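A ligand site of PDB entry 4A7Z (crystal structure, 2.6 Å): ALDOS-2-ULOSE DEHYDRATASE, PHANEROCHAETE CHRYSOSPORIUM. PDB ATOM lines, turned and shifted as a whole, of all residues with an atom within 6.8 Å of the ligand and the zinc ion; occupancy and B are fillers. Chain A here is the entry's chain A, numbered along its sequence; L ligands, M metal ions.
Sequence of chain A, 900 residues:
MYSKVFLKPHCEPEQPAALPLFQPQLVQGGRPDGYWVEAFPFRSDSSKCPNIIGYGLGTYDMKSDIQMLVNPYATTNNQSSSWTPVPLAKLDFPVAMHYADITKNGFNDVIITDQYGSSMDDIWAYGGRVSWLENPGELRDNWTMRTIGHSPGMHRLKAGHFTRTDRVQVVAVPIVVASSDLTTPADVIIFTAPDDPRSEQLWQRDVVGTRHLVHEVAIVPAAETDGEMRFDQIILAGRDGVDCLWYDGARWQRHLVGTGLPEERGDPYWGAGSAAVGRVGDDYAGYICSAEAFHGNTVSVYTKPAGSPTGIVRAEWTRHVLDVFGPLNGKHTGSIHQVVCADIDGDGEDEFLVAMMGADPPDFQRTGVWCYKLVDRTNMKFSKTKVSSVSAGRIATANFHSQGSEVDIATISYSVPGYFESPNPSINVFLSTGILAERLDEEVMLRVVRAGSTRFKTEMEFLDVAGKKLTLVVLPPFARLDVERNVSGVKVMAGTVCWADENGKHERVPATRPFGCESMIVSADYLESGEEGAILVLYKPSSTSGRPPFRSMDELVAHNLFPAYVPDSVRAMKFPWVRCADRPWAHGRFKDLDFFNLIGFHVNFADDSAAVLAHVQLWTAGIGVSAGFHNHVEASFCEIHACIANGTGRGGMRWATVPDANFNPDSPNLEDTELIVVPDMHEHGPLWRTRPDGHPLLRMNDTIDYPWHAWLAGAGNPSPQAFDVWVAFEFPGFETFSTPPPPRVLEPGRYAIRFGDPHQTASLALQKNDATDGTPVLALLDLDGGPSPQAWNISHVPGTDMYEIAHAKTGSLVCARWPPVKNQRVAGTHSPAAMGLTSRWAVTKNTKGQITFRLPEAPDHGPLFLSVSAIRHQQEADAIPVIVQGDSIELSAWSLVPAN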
ATOM      1  N   TYR A  35     -12.925 -13.982 -13.655  1.00  0.00           N
ATOM      2  CA  TYR A  35     -11.813 -13.087 -14.013  1.00  0.00           C
ATOM      3  C   TYR A  35     -11.781 -11.718 -13.320  1.00  0.00           C
ATOM      4  O   TYR A  35     -10.740 -11.310 -12.819  1.00  0.00           O
ATOM      5  CB  TYR A  35     -11.838 -12.812 -15.513  1.00  0.00           C
ATOM      6  CG  TYR A  35     -10.604 -12.087 -15.951  1.00  0.00           C
ATOM      7  CD1 TYR A  35      -9.386 -12.784 -16.009  1.00  0.00           C
ATOM      8  CD2 TYR A  35     -10.616 -10.737 -16.292  1.00  0.00           C
ATOM      9  CE1 TYR A  35      -8.231 -12.146 -16.414  1.00  0.00           C
ATOM     10  CE2 TYR A  35      -9.429 -10.100 -16.715  1.00  0.00           C
ATOM     11  CZ  TYR A  35      -8.254 -10.826 -16.760  1.00  0.00           C
ATOM     12  OH  TYR A  35      -7.073 -10.278 -17.159  1.00  0.00           O
ATOM     13  N   LEU A  57     -14.207 -14.163 -19.168  1.00  0.00           N
ATOM     14  CA  LEU A  57     -14.021 -13.786 -20.561  1.00  0.00           C
ATOM     15  C   LEU A  57     -15.059 -14.450 -21.480  1.00  0.00           C
ATOM     16  O   LEU A  57     -15.192 -14.072 -22.644  1.00  0.00           O
ATOM     17  CB  LEU A  57     -12.613 -14.172 -21.049  1.00  0.00           C
ATOM     18  CG  LEU A  57     -11.263 -13.635 -20.582  1.00  0.00           C
ATOM     19  CD1 LEU A  57     -10.455 -13.414 -21.847  1.00  0.00           C
ATOM     20  CD2 LEU A  57     -11.287 -12.350 -19.769  1.00  0.00           C
ATOM     21  N   VAL A  95     -12.780  -7.915 -20.899  1.00  0.00           N
ATOM     22  CA  VAL A  95     -11.612  -8.082 -20.056  1.00  0.00           C
ATOM     23  C   VAL A  95     -11.660  -7.155 -18.865  1.00  0.00           C
ATOM     24  O   VAL A  95     -12.117  -7.558 -17.834  1.00  0.00           O
ATOM     25  CB  VAL A  95     -10.247  -7.966 -20.793  1.00  0.00           C
ATOM     26  CG1 VAL A  95      -9.108  -8.070 -19.789  1.00  0.00           C
ATOM     27  CG2 VAL A  95     -10.102  -9.058 -21.819  1.00  0.00           C
ATOM     28  N   TYR A 116     -11.945  -8.880 -27.089  1.00  0.00           N
ATOM     29  CA  TYR A 116     -10.510  -9.025 -26.896  1.00  0.00           C
ATOM     30  C   TYR A 116      -9.946 -10.182 -27.711  1.00  0.00           C
ATOM     31  O   TYR A 116      -9.002 -10.027 -28.493  1.00  0.00           O
ATOM     32  CB  TYR A 116     -10.241  -9.249 -25.420  1.00  0.00           C
ATOM     33  CG  TYR A 116      -8.824  -9.589 -25.043  1.00  0.00           C
ATOM     34  CD1 TYR A 116      -7.864  -8.603 -24.959  1.00  0.00           C
ATOM     35  CD2 TYR A 116      -8.445 -10.893 -24.718  1.00  0.00           C
ATOM     36  CE1 TYR A 116      -6.572  -8.880 -24.560  1.00  0.00           C
ATOM     37  CE2 TYR A 116      -7.151 -11.199 -24.329  1.00  0.00           C
ATOM     38  CZ  TYR A 116      -6.204 -10.179 -24.243  1.00  0.00           C
ATOM     39  OH  TYR A 116      -4.871 -10.405 -23.877  1.00  0.00           O
ATOM     40  N   GLY A 117     -10.540 -11.353 -27.504  1.00  0.00           N
ATOM     41  CA  GLY A 117     -10.101 -12.603 -28.107  1.00  0.00           C
ATOM     42  C   GLY A 117     -10.028 -13.551 -26.955  1.00  0.00           C
ATOM     43  O   GLY A 117     -10.379 -13.168 -25.836  1.00  0.00           O
ATOM     44  N   SER A 118      -9.578 -14.786 -27.199  1.00  0.00           N
ATOM     45  CA  SER A 118      -9.477 -15.765 -26.105  1.00  0.00           C
ATOM     46  C   SER A 118      -8.115 -15.814 -25.368  1.00  0.00           C
ATOM     47  O   SER A 118      -8.016 -16.340 -24.264  1.00  0.00           O
ATOM     48  CB  SER A 118      -9.863 -17.161 -26.580  1.00  0.00           C
ATOM     49  OG  SER A 118      -8.742 -17.777 -27.162  1.00  0.00           O
ATOM     50  N   SER A 119      -7.066 -15.292 -25.970  1.00  0.00           N
ATOM     51  CA  SER A 119      -5.751 -15.333 -25.345  1.00  0.00           C
ATOM     52  C   SER A 119      -4.768 -14.403 -26.073  1.00  0.00           C
ATOM     53  O   SER A 119      -5.071 -13.857 -27.144  1.00  0.00           O
ATOM     54  CB  SER A 119      -5.225 -16.784 -25.324  1.00  0.00           C
ATOM     55  OG  SER A 119      -4.857 -17.239 -26.622  1.00  0.00           O
ATOM     56  N   MET A 120      -3.584 -14.244 -25.491  1.00  0.00           N
ATOM     57  CA  MET A 120      -2.499 -13.484 -26.128  1.00  0.00           C
ATOM     58  C   MET A 120      -2.060 -14.135 -27.439  1.00  0.00           C
ATOM     59  O   MET A 120      -1.329 -13.537 -28.227  1.00  0.00           O
ATOM     60  CB  MET A 120      -1.330 -13.273 -25.150  1.00  0.00           C
ATOM     61  CG  MET A 120      -1.629 -12.150 -24.177  1.00  0.00           C
ATOM     62  SD  MET A 120      -0.807 -12.254 -22.581  1.00  0.00           S
ATOM     63  CE  MET A 120       0.852 -11.768 -23.043  1.00  0.00           C
ATOM     64  N   ASP A 121      -2.527 -15.365 -27.658  1.00  0.00           N
ATOM     65  CA  ASP A 121      -2.279 -16.067 -28.886  1.00  0.00           C
ATOM     66  C   ASP A 121      -3.462 -15.987 -29.847  1.00  0.00           C
ATOM     67  O   ASP A 121      -3.354 -16.385 -30.994  1.00  0.00           O
ATOM     68  CB  ASP A 121      -1.904 -17.530 -28.577  1.00  0.00           C
ATOM     69  CG  ASP A 121      -0.501 -17.654 -28.015  1.00  0.00           C
ATOM     70  OD1 ASP A 121       0.452 -17.121 -28.633  1.00  0.00           O
ATOM     71  OD2 ASP A 121      -0.341 -18.290 -26.956  1.00  0.00           O
ATOM     72  N   ILE A 123      -5.685 -12.967 -30.563  1.00  0.00           N
ATOM     73  CA  ILE A 123      -6.073 -11.553 -30.433  1.00  0.00           C
ATOM     74  C   ILE A 123      -6.902 -11.136 -31.641  1.00  0.00           C
ATOM     75  O   ILE A 123      -6.509 -11.390 -32.763  1.00  0.00           O
ATOM     76  CB  ILE A 123      -4.846 -10.627 -30.315  1.00  0.00           C
ATOM     77  CG1 ILE A 123      -4.049 -10.929 -29.060  1.00  0.00           C
ATOM     78  CG2 ILE A 123      -5.262  -9.172 -30.313  1.00  0.00           C
ATOM     79  CD1 ILE A 123      -4.592 -10.281 -27.804  1.00  0.00           C
ATOM     80  N   HIS A 155      -6.615  -4.318 -22.932  1.00  0.00           N
ATOM     81  CA  HIS A 155      -6.544  -5.274 -21.820  1.00  0.00           C
ATOM     82  C   HIS A 155      -6.710  -4.712 -20.413  1.00  0.00           C
ATOM     83  O   HIS A 155      -6.996  -5.477 -19.470  1.00  0.00           O
ATOM     84  CB  HIS A 155      -5.246  -6.068 -21.979  1.00  0.00           C
ATOM     85  CG  HIS A 155      -4.878  -6.886 -20.774  1.00  0.00           C
ATOM     86  ND1 HIS A 155      -4.302  -6.332 -19.688  1.00  0.00           N
ATOM     87  CD2 HIS A 155      -4.990  -8.243 -20.514  1.00  0.00           C
ATOM     88  CE1 HIS A 155      -4.060  -7.295 -18.776  1.00  0.00           C
ATOM     89  NE2 HIS A 155      -4.502  -8.464 -19.272  1.00  0.00           N
ATOM     90  N   ARG A 156      -6.520  -3.402 -20.227  1.00  0.00           N
ATOM     91  CA  ARG A 156      -6.753  -2.749 -18.949  1.00  0.00           C
ATOM     92  C   ARG A 156      -7.190  -1.320 -19.210  1.00  0.00           C
ATOM     93  O   ARG A 156      -6.803  -0.722 -20.227  1.00  0.00           O
ATOM     94  CB  ARG A 156      -5.479  -2.717 -18.098  1.00  0.00           C
ATOM     95  CG  ARG A 156      -5.067  -4.002 -17.441  1.00  0.00           C
ATOM     96  CD  ARG A 156      -6.144  -4.501 -16.512  1.00  0.00           C
ATOM     97  NE  ARG A 156      -5.713  -5.670 -15.760  1.00  0.00           N
ATOM     98  CZ  ARG A 156      -5.932  -6.916 -16.147  1.00  0.00           C
ATOM     99  NH1 ARG A 156      -6.514  -7.152 -17.312  1.00  0.00           N
ATOM    100  NH2 ARG A 156      -5.544  -7.934 -15.397  1.00  0.00           N
ATOM    101  N   ILE A 175      -2.192  -5.097 -23.972  1.00  0.00           N
ATOM    102  CA  ILE A 175      -1.081  -5.800 -23.380  1.00  0.00           C
ATOM    103  C   ILE A 175      -0.171  -6.211 -24.491  1.00  0.00           C
ATOM    104  O   ILE A 175       1.037  -6.246 -24.314  1.00  0.00           O
ATOM    105  CB  ILE A 175      -1.528  -7.037 -22.538  1.00  0.00           C
ATOM    106  CG1 ILE A 175      -0.297  -7.650 -21.825  1.00  0.00           C
ATOM    107  CG2 ILE A 175      -2.336  -8.056 -23.375  1.00  0.00           C
ATOM    108  CD1 ILE A 175      -0.595  -8.720 -20.809  1.00  0.00           C
ATOM    109  N   VAL A 176      -0.768  -6.580 -25.638  1.00  0.00           N
ATOM    110  CA  VAL A 176      -0.006  -6.943 -26.876  1.00  0.00           C
ATOM    111  C   VAL A 176      -0.845  -6.364 -28.034  1.00  0.00           C
ATOM    112  O   VAL A 176      -2.058  -6.044 -27.834  1.00  0.00           O
ATOM    113  CB  VAL A 176       0.255  -8.481 -27.012  1.00  0.00           C
ATOM    114  CG1 VAL A 176       1.059  -9.010 -25.836  1.00  0.00           C
ATOM    115  CG2 VAL A 176      -1.040  -9.304 -27.145  1.00  0.00           C
ATOM    116  N   HIS A 215       0.365  -4.892 -17.825  1.00  0.00           N
ATOM    117  CA  HIS A 215      -0.628  -5.834 -17.311  1.00  0.00           C
ATOM    118  C   HIS A 215      -1.519  -5.230 -16.272  1.00  0.00           C
ATOM    119  O   HIS A 215      -2.526  -5.840 -15.907  1.00  0.00           O
ATOM    120  CB  HIS A 215       0.034  -7.113 -16.772  1.00  0.00           C
ATOM    121  CG  HIS A 215      -0.965  -8.142 -16.286  1.00  0.00           C
ATOM    122  ND1 HIS A 215      -1.231  -8.336 -14.979  1.00  0.00           N
ATOM    123  CD2 HIS A 215      -1.783  -9.007 -17.000  1.00  0.00           C
ATOM    124  CE1 HIS A 215      -2.175  -9.281 -14.861  1.00  0.00           C
ATOM    125  NE2 HIS A 215      -2.515  -9.702 -16.085  1.00  0.00           N
ATOM    126  N   PHE A 294       4.714 -10.740 -15.213  1.00  0.00           N
ATOM    127  CA  PHE A 294       3.403 -11.155 -15.673  1.00  0.00           C
ATOM    128  C   PHE A 294       3.011 -12.535 -15.111  1.00  0.00           C
ATOM    129  O   PHE A 294       3.693 -13.561 -15.371  1.00  0.00           O
ATOM    130  CB  PHE A 294       3.457 -11.239 -17.186  1.00  0.00           C
ATOM    131  CG  PHE A 294       2.273 -11.900 -17.787  1.00  0.00           C
ATOM    132  CD1 PHE A 294       1.035 -11.212 -17.838  1.00  0.00           C
ATOM    133  CD2 PHE A 294       2.376 -13.178 -18.301  1.00  0.00           C
ATOM    134  CE1 PHE A 294      -0.068 -11.810 -18.400  1.00  0.00           C
ATOM    135  CE2 PHE A 294       1.283 -13.795 -18.865  1.00  0.00           C
ATOM    136  CZ  PHE A 294       0.056 -13.112 -18.908  1.00  0.00           C
ATOM    137  N   HIS A 295       1.906 -12.539 -14.353  1.00  0.00           N
ATOM    138  CA  HIS A 295       1.373 -13.759 -13.705  1.00  0.00           C
ATOM    139  C   HIS A 295       2.474 -14.460 -12.956  1.00  0.00           C
ATOM    140  O   HIS A 295       2.531 -15.680 -12.910  1.00  0.00           O
ATOM    141  CB  HIS A 295       0.764 -14.708 -14.752  1.00  0.00           C
ATOM    142  CG  HIS A 295      -0.471 -14.169 -15.421  1.00  0.00           C
ATOM    143  ND1 HIS A 295      -1.341 -14.974 -16.061  1.00  0.00           N
ATOM    144  CD2 HIS A 295      -0.965 -12.869 -15.539  1.00  0.00           C
ATOM    145  CE1 HIS A 295      -2.338 -14.223 -16.580  1.00  0.00           C
ATOM    146  NE2 HIS A 295      -2.091 -12.935 -16.253  1.00  0.00           N
ATOM    147  N   HIS A 337      -1.836 -12.616  -9.623  1.00  0.00           N
ATOM    148  CA  HIS A 337      -2.452 -11.804 -10.700  1.00  0.00           C
ATOM    149  C   HIS A 337      -2.571 -10.322 -10.436  1.00  0.00           C
ATOM    150  O   HIS A 337      -2.614  -9.517 -11.355  1.00  0.00           O
ATOM    151  CB  HIS A 337      -3.837 -12.335 -11.075  1.00  0.00           C
ATOM    152  CG  HIS A 337      -4.287 -11.916 -12.477  1.00  0.00           C
ATOM    153  ND1 HIS A 337      -5.459 -11.283 -12.709  1.00  0.00           N
ATOM    154  CD2 HIS A 337      -3.686 -12.086 -13.709  1.00  0.00           C
ATOM    155  CE1 HIS A 337      -5.605 -11.063 -14.032  1.00  0.00           C
ATOM    156  NE2 HIS A 337      -4.517 -11.540 -14.640  1.00  0.00           N
ATOM    157  N   MET A 357      -4.057 -16.700  -7.609  1.00  0.00           N
ATOM    158  CA  MET A 357      -4.866 -17.429  -8.577  1.00  0.00           C
ATOM    159  C   MET A 357      -5.069 -18.891  -8.229  1.00  0.00           C
ATOM    160  O   MET A 357      -6.154 -19.421  -8.456  1.00  0.00           O
ATOM    161  CB  MET A 357      -4.200 -17.375  -9.935  1.00  0.00           C
ATOM    162  CG  MET A 357      -3.948 -15.960 -10.357  1.00  0.00           C
ATOM    163  SD  MET A 357      -3.201 -16.009 -11.951  1.00  0.00           S
ATOM    164  CE  MET A 357      -1.487 -16.302 -11.571  1.00  0.00           C
ATOM    165  N   TYR A 414      -9.971 -17.121 -10.201  1.00  0.00           N
ATOM    166  CA  TYR A 414      -9.300 -17.018 -11.479  1.00  0.00           C
ATOM    167  C   TYR A 414      -9.575 -18.264 -12.296  1.00  0.00           C
ATOM    168  O   TYR A 414      -9.004 -19.338 -12.007  1.00  0.00           O
ATOM    169  CB  TYR A 414      -7.758 -16.885 -11.301  1.00  0.00           C
ATOM    170  CG  TYR A 414      -7.151 -16.491 -12.610  1.00  0.00           C
ATOM    171  CD1 TYR A 414      -6.876 -17.445 -13.611  1.00  0.00           C
ATOM    172  CD2 TYR A 414      -6.971 -15.149 -12.908  1.00  0.00           C
ATOM    173  CE1 TYR A 414      -6.387 -17.045 -14.858  1.00  0.00           C
ATOM    174  CE2 TYR A 414      -6.490 -14.752 -14.131  1.00  0.00           C
ATOM    175  CZ  TYR A 414      -6.202 -15.683 -15.096  1.00  0.00           C
ATOM    176  OH  TYR A 414      -5.713 -15.170 -16.262  1.00  0.00           O
ATOM    177  N   VAL A 416      -9.655 -18.999 -16.417  1.00  0.00           N
ATOM    178  CA  VAL A 416      -9.570 -18.512 -17.776  1.00  0.00           C
ATOM    179  C   VAL A 416      -8.967 -19.611 -18.654  1.00  0.00           C
ATOM    180  O   VAL A 416      -7.790 -19.938 -18.524  1.00  0.00           O
ATOM    181  CB  VAL A 416      -8.751 -17.189 -17.870  1.00  0.00           C
ATOM    182  CG1 VAL A 416      -8.636 -16.716 -19.320  1.00  0.00           C
ATOM    183  CG2 VAL A 416      -9.392 -16.096 -17.024  1.00  0.00           C
ATOM    184  N   PRO A 417      -9.780 -20.162 -19.543  1.00  0.00           N
ATOM    185  CA  PRO A 417      -9.286 -21.134 -20.519  1.00  0.00           C
ATOM    186  C   PRO A 417      -7.902 -20.767 -21.092  1.00  0.00           C
ATOM    187  O   PRO A 417      -7.735 -19.674 -21.639  1.00  0.00           O
ATOM    188  CB  PRO A 417     -10.374 -21.105 -21.608  1.00  0.00           C
ATOM    189  CG  PRO A 417     -11.631 -20.778 -20.848  1.00  0.00           C
ATOM    190  CD  PRO A 417     -11.226 -19.883 -19.715  1.00  0.00           C
ATOM    191  N   TYR A 419      -4.861 -20.643 -19.335  1.00  0.00           N
ATOM    192  CA  TYR A 419      -3.970 -19.993 -18.366  1.00  0.00           C
ATOM    193  C   TYR A 419      -3.945 -20.753 -17.040  1.00  0.00           C
ATOM    194  O   TYR A 419      -2.899 -21.291 -16.631  1.00  0.00           O
ATOM    195  CB  TYR A 419      -4.448 -18.569 -18.119  1.00  0.00           C
ATOM    196  CG  TYR A 419      -4.153 -17.668 -19.264  1.00  0.00           C
ATOM    197  CD1 TYR A 419      -5.053 -17.541 -20.333  1.00  0.00           C
ATOM    198  CD2 TYR A 419      -2.945 -16.957 -19.312  1.00  0.00           C
ATOM    199  CE1 TYR A 419      -4.757 -16.713 -21.414  1.00  0.00           C
ATOM    200  CE2 TYR A 419      -2.652 -16.138 -20.383  1.00  0.00           C
ATOM    201  CZ  TYR A 419      -3.552 -16.018 -21.430  1.00  0.00           C
ATOM    202  OH  TYR A 419      -3.236 -15.223 -22.486  1.00  0.00           O
HETATM  203  C1  LIG L   1      -6.165 -13.316 -18.764  1.00  0.00           C
HETATM  204  C2  LIG L   1      -5.263 -12.469 -18.166  1.00  0.00           C
HETATM  205  C3  LIG L   1      -4.460 -11.691 -18.977  1.00  0.00           C
HETATM  206  C4  LIG L   1      -4.562 -11.756 -20.366  1.00  0.00           C
HETATM  207  C5  LIG L   1      -5.559 -12.587 -20.889  1.00  0.00           C
HETATM  208  C6  LIG L   1      -5.404 -13.144 -22.251  1.00  0.00           C
HETATM  209  O1  LIG L   1      -5.117 -12.442 -16.942  1.00  0.00           O
HETATM  210  O2  LIG L   1      -3.609 -10.846 -18.375  1.00  0.00           O
HETATM  211  O3  LIG L   1      -5.785 -13.733 -20.076  1.00  0.00           O
HETATM  212  O4  LIG L   1      -4.051 -12.946 -22.615  1.00  0.00           O
HETATM  213 ZN    ZN M   1      -3.665 -11.471 -16.399  1.00  0.00          ZN
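Ser 119 touches the ligand. CE1 of Phe 294 touches O2 of the ligand, at 3.7 Å. Hydrophobic or aromatic side chains within 4 Å of the ligand: Tyr 35, Tyr 116, Met 120, His 155, His 215, Phe 294, His 295, His 337, Tyr 414 and Tyr 419. 11 residues have an atom within 4 Å of the ligand: Tyr 35, Tyr 116, Ser 119, Met 120, His 155, His 215, Phe 294, His 295, His 337, Tyr 414 and Tyr 419.
The zinc ion is bound by an oxygen (O1) of the ligand (1.8 Å), a ring nitrogen (NE2) of His 337 (2.0 Å), an oxygen (O2) of the ligand (2.1 Å), a ring nitrogen (NE2) of His 215 (2.1 Å) and a ring nitrogen (NE2) of His 295 (2.2 Å). The zinc ion has five donor atoms within binding distance.
OH of Tyr 35 touches the zinc ion, at 3.7 Å. Of the 23 residues printed, 4 come within 4 Å of the zinc ion. The nearest printed residue that does not touch the zinc ion is Arg 156 (4.1 Å).
An oxygen (O4) of the ligand is in hydrogen-bond range of the side-chain hydroxyl (OH) of Tyr 419, at 2.4 Å. A ring nitrogen (NE2) of His 155 lies close to an oxygen (O2) of the ligand, at 2.7 Å. An oxygen (O1) of the ligand lies close to the side-chain hydroxyl (OH) of Tyr 414, at 2.9 Å. An oxygen (O1) of the ligand sits close to the side-chain hydroxyl of Tyr 35 (2.9 Å). O4 of the ligand sits at hydrogen-bond distance from OH of Tyr 116, at 3.0 Å. N of Met 120 lies close to O4 of the ligand (3.2 Å). O4 of the ligand sits close to SD of Met 120 (3.3 Å).
The guanidinium group (NE) of Arg 156 lies within hydrogen-bond range of the backbone carbonyl oxygen (O) of His 215, 3.2 Å away. The side-chain hydroxyl (OH) of Tyr 419 sits at hydrogen-bond distance from the backbone NH (N) of Met 120 (3.2 Å). A ring nitrogen (NE2) of His 155 lies close to the guanidinium group (NH1) of Arg 156 (3.1 Å). The side-chain hydroxyl (OH) of Tyr 35 lies within hydrogen-bond range of the guanidinium group (NH1) of Arg 156 (3.2 Å). N of Asp 121 sits close to OG of Ser 119 (3.2 Å).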
